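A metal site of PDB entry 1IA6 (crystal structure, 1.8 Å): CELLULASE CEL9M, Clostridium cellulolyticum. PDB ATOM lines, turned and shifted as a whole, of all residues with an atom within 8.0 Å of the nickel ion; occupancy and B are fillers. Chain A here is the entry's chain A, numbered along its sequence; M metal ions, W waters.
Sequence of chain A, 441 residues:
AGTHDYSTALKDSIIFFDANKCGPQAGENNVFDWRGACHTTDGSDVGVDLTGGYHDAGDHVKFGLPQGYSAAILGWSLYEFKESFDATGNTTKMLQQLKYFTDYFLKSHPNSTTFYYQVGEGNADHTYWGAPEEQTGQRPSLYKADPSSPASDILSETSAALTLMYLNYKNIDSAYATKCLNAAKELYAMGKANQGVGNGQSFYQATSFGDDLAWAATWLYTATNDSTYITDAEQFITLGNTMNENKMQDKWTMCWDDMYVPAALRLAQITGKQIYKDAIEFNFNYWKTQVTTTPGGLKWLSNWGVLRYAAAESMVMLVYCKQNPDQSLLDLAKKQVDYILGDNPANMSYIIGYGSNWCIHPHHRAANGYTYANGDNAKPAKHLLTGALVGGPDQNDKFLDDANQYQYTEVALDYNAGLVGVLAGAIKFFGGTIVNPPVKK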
ATOM      1  N   ALA A   1      20.268 -24.647   7.650  1.00  0.00           N
ATOM      2  CA  ALA A   1      19.407 -25.443   8.564  1.00  0.00           C
ATOM      3  C   ALA A   1      18.589 -26.462   7.779  1.00  0.00           C
ATOM      4  O   ALA A   1      18.100 -26.174   6.680  1.00  0.00           O
ATOM      5  CB  ALA A   1      18.475 -24.517   9.336  1.00  0.00           C
ATOM      6  N   GLY A   2      18.424 -27.650   8.350  1.00  0.00           N
ATOM      7  CA  GLY A   2      17.672 -28.698   7.690  1.00  0.00           C
ATOM      8  C   GLY A   2      16.250 -28.274   7.346  1.00  0.00           C
ATOM      9  O   GLY A   2      15.731 -28.636   6.294  1.00  0.00           O
ATOM     10  N   THR A   3      15.633 -27.510   8.234  1.00  0.00           N
ATOM     11  CA  THR A   3      14.269 -27.044   8.015  1.00  0.00           C
ATOM     12  C   THR A   3      14.140 -25.554   8.331  1.00  0.00           C
ATOM     13  O   THR A   3      14.848 -25.031   9.193  1.00  0.00           O
ATOM     14  CB  THR A   3      13.273 -27.823   8.897  1.00  0.00           C
ATOM     15  OG1 THR A   3      11.939 -27.409   8.583  1.00  0.00           O
ATOM     16  CG2 THR A   3      13.552 -27.562  10.376  1.00  0.00           C
ATOM     17  N   HIS A   4      13.247 -24.874   7.620  1.00  0.00           N
ATOM     18  CA  HIS A   4      13.022 -23.442   7.808  1.00  0.00           C
ATOM     19  C   HIS A   4      11.542 -23.127   7.942  1.00  0.00           C
ATOM     20  O   HIS A   4      10.695 -23.821   7.375  1.00  0.00           O
ATOM     21  CB  HIS A   4      13.615 -22.660   6.623  1.00  0.00           C
ATOM     22  CG  HIS A   4      15.107 -22.637   6.602  1.00  0.00           C
ATOM     23  ND1 HIS A   4      15.839 -21.777   7.396  1.00  0.00           N
ATOM     24  CD2 HIS A   4      16.001 -23.366   5.910  1.00  0.00           C
ATOM     25  CE1 HIS A   4      17.131 -21.998   7.194  1.00  0.00           C
ATOM     26  NE2 HIS A   4      17.258 -22.962   6.297  1.00  0.00           N
ATOM     27  N   TYR A   6       9.115 -21.000   6.705  1.00  0.00           N
ATOM     28  CA  TYR A   6       8.736 -20.045   5.664  1.00  0.00           C
ATOM     29  C   TYR A   6       7.383 -19.404   5.952  1.00  0.00           C
ATOM     30  O   TYR A   6       7.124 -18.276   5.538  1.00  0.00           O
ATOM     31  CB  TYR A   6       8.674 -20.737   4.300  1.00  0.00           C
ATOM     32  CG  TYR A   6       9.971 -21.393   3.876  1.00  0.00           C
ATOM     33  CD1 TYR A   6      11.121 -20.630   3.661  1.00  0.00           C
ATOM     34  CD2 TYR A   6      10.059 -22.774   3.707  1.00  0.00           C
ATOM     35  CE1 TYR A   6      12.320 -21.234   3.277  1.00  0.00           C
ATOM     36  CE2 TYR A   6      11.249 -23.382   3.337  1.00  0.00           C
ATOM     37  CZ  TYR A   6      12.376 -22.608   3.124  1.00  0.00           C
ATOM     38  OH  TYR A   6      13.556 -23.220   2.767  1.00  0.00           O
ATOM     39  N   LYS A 334      15.966 -21.483  -3.589  1.00  0.00           N
ATOM     40  CA  LYS A 334      15.930 -21.927  -2.207  1.00  0.00           C
ATOM     41  C   LYS A 334      17.153 -21.463  -1.429  1.00  0.00           C
ATOM     42  O   LYS A 334      17.040 -21.106  -0.262  1.00  0.00           O
ATOM     43  CB  LYS A 334      15.813 -23.449  -2.111  1.00  0.00           C
ATOM     44  CG  LYS A 334      15.516 -23.943  -0.716  1.00  0.00           C
ATOM     45  CD  LYS A 334      15.355 -25.463  -0.671  1.00  0.00           C
ATOM     46  CE  LYS A 334      14.827 -25.921   0.681  1.00  0.00           C
ATOM     47  NZ  LYS A 334      15.753 -25.599   1.797  1.00  0.00           N
ATOM     48  N   LYS A 335      18.315 -21.465  -2.064  1.00  0.00           N
ATOM     49  CA  LYS A 335      19.531 -21.040  -1.382  1.00  0.00           C
ATOM     50  C   LYS A 335      19.482 -19.549  -1.039  1.00  0.00           C
ATOM     51  O   LYS A 335      19.936 -19.144   0.024  1.00  0.00           O
ATOM     52  CB  LYS A 335      20.758 -21.347  -2.240  1.00  0.00           C
ATOM     53  CG  LYS A 335      21.070 -22.831  -2.347  1.00  0.00           C
ATOM     54  CD  LYS A 335      22.388 -23.074  -3.073  1.00  0.00           C
ATOM     55  CE  LYS A 335      22.727 -24.558  -3.132  1.00  0.00           C
ATOM     56  NZ  LYS A 335      24.044 -24.784  -3.803  1.00  0.00           N
ATOM     57  N   VAL A 337      16.730 -17.711  -0.532  1.00  0.00           N
ATOM     58  CA  VAL A 337      15.760 -17.528   0.528  1.00  0.00           C
ATOM     59  C   VAL A 337      16.325 -17.962   1.870  1.00  0.00           C
ATOM     60  O   VAL A 337      16.225 -17.241   2.868  1.00  0.00           O
ATOM     61  CB  VAL A 337      14.465 -18.330   0.269  1.00  0.00           C
ATOM     62  CG1 VAL A 337      13.531 -18.202   1.454  1.00  0.00           C
ATOM     63  CG2 VAL A 337      13.794 -17.819  -0.994  1.00  0.00           C
ATOM     64  N   ASP A 338      16.927 -19.154   1.905  1.00  0.00           N
ATOM     65  CA  ASP A 338      17.490 -19.662   3.144  1.00  0.00           C
ATOM     66  C   ASP A 338      18.605 -18.773   3.679  1.00  0.00           C
ATOM     67  O   ASP A 338      18.778 -18.652   4.892  1.00  0.00           O
ATOM     68  CB  ASP A 338      17.997 -21.098   2.957  1.00  0.00           C
ATOM     69  CG  ASP A 338      16.872 -22.093   2.717  1.00  0.00           C
ATOM     70  OD1 ASP A 338      15.698 -21.717   2.930  1.00  0.00           O
ATOM     71  OD2 ASP A 338      17.160 -23.235   2.330  1.00  0.00           O
ATOM     72  N   TYR A 339      19.343 -18.139   2.778  1.00  0.00           N
ATOM     73  CA  TYR A 339      20.416 -17.235   3.172  1.00  0.00           C
ATOM     74  C   TYR A 339      19.801 -16.049   3.922  1.00  0.00           C
ATOM     75  O   TYR A 339      20.286 -15.648   4.984  1.00  0.00           O
ATOM     76  CB  TYR A 339      21.185 -16.748   1.946  1.00  0.00           C
ATOM     77  CG  TYR A 339      22.357 -15.836   2.246  1.00  0.00           C
ATOM     78  CD1 TYR A 339      22.158 -14.508   2.611  1.00  0.00           C
ATOM     79  CD2 TYR A 339      23.676 -16.315   2.162  1.00  0.00           C
ATOM     80  CE1 TYR A 339      23.246 -13.668   2.889  1.00  0.00           C
ATOM     81  CE2 TYR A 339      24.757 -15.481   2.440  1.00  0.00           C
ATOM     82  CZ  TYR A 339      24.539 -14.162   2.797  1.00  0.00           C
ATOM     83  OH  TYR A 339      25.603 -13.325   3.072  1.00  0.00           O
ATOM     84  N   LEU A 341      16.974 -15.952   5.498  1.00  0.00           N
ATOM     85  CA  LEU A 341      16.400 -16.404   6.754  1.00  0.00           C
ATOM     86  C   LEU A 341      17.410 -16.727   7.860  1.00  0.00           C
ATOM     87  O   LEU A 341      17.025 -16.910   9.022  1.00  0.00           O
ATOM     88  CB  LEU A 341      15.498 -17.610   6.516  1.00  0.00           C
ATOM     89  CG  LEU A 341      14.282 -17.352   5.617  1.00  0.00           C
ATOM     90  CD1 LEU A 341      13.505 -18.640   5.385  1.00  0.00           C
ATOM     91  CD2 LEU A 341      13.394 -16.296   6.255  1.00  0.00           C
ATOM     92  N   GLY A 342      18.691 -16.830   7.517  1.00  0.00           N
ATOM     93  CA  GLY A 342      19.670 -17.118   8.546  1.00  0.00           C
ATOM     94  C   GLY A 342      20.834 -18.017   8.183  1.00  0.00           C
ATOM     95  O   GLY A 342      21.793 -18.132   8.935  1.00  0.00           O
ATOM     96  N   ASP A 343      20.753 -18.683   7.037  1.00  0.00           N
ATOM     97  CA  ASP A 343      21.821 -19.578   6.586  1.00  0.00           C
ATOM     98  C   ASP A 343      22.929 -18.773   5.927  1.00  0.00           C
ATOM     99  O   ASP A 343      23.102 -18.835   4.707  1.00  0.00           O
ATOM    100  CB  ASP A 343      21.279 -20.583   5.579  1.00  0.00           C
ATOM    101  CG  ASP A 343      20.583 -21.754   6.233  1.00  0.00           C
ATOM    102  OD1 ASP A 343      20.204 -21.654   7.414  1.00  0.00           O
ATOM    103  OD2 ASP A 343      20.413 -22.785   5.543  1.00  0.00           O
ATOM    104  N   ASN A 344      23.691 -18.024   6.718  1.00  0.00           N
ATOM    105  CA  ASN A 344      24.762 -17.204   6.175  1.00  0.00           C
ATOM    106  C   ASN A 344      25.919 -17.089   7.162  1.00  0.00           C
ATOM    107  O   ASN A 344      25.787 -17.410   8.345  1.00  0.00           O
ATOM    108  CB  ASN A 344      24.217 -15.808   5.833  1.00  0.00           C
ATOM    109  CG  ASN A 344      23.521 -15.163   7.015  1.00  0.00           C
ATOM    110  OD1 ASN A 344      24.161 -14.864   8.026  1.00  0.00           O
ATOM    111  ND2 ASN A 344      22.214 -14.944   6.895  1.00  0.00           N
HETATM  112 NI    NI M   1      19.003 -24.099   5.989  1.00  0.00          NI
HETATM  113  O   HOH W   1      18.880 -24.955   4.073  1.00  0.00           O
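N of Asp 343 sits at hydrogen-bond distance from O of Asp 338, at 2.9 Å.
The nickel ion is bound by OD2 of Asp 343 (2.0 Å).
Water W1 binds the nickel ion, 2.1 Å away.
NE2 of His 4 binds the nickel ion (2.1 Å).
N of Ala 1 is bound to the nickel ion.
O of Ala 1 is bound to the nickel ion.
Within 4 Å of the nickel ion: Ala 1, His 4 and Asp 343.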
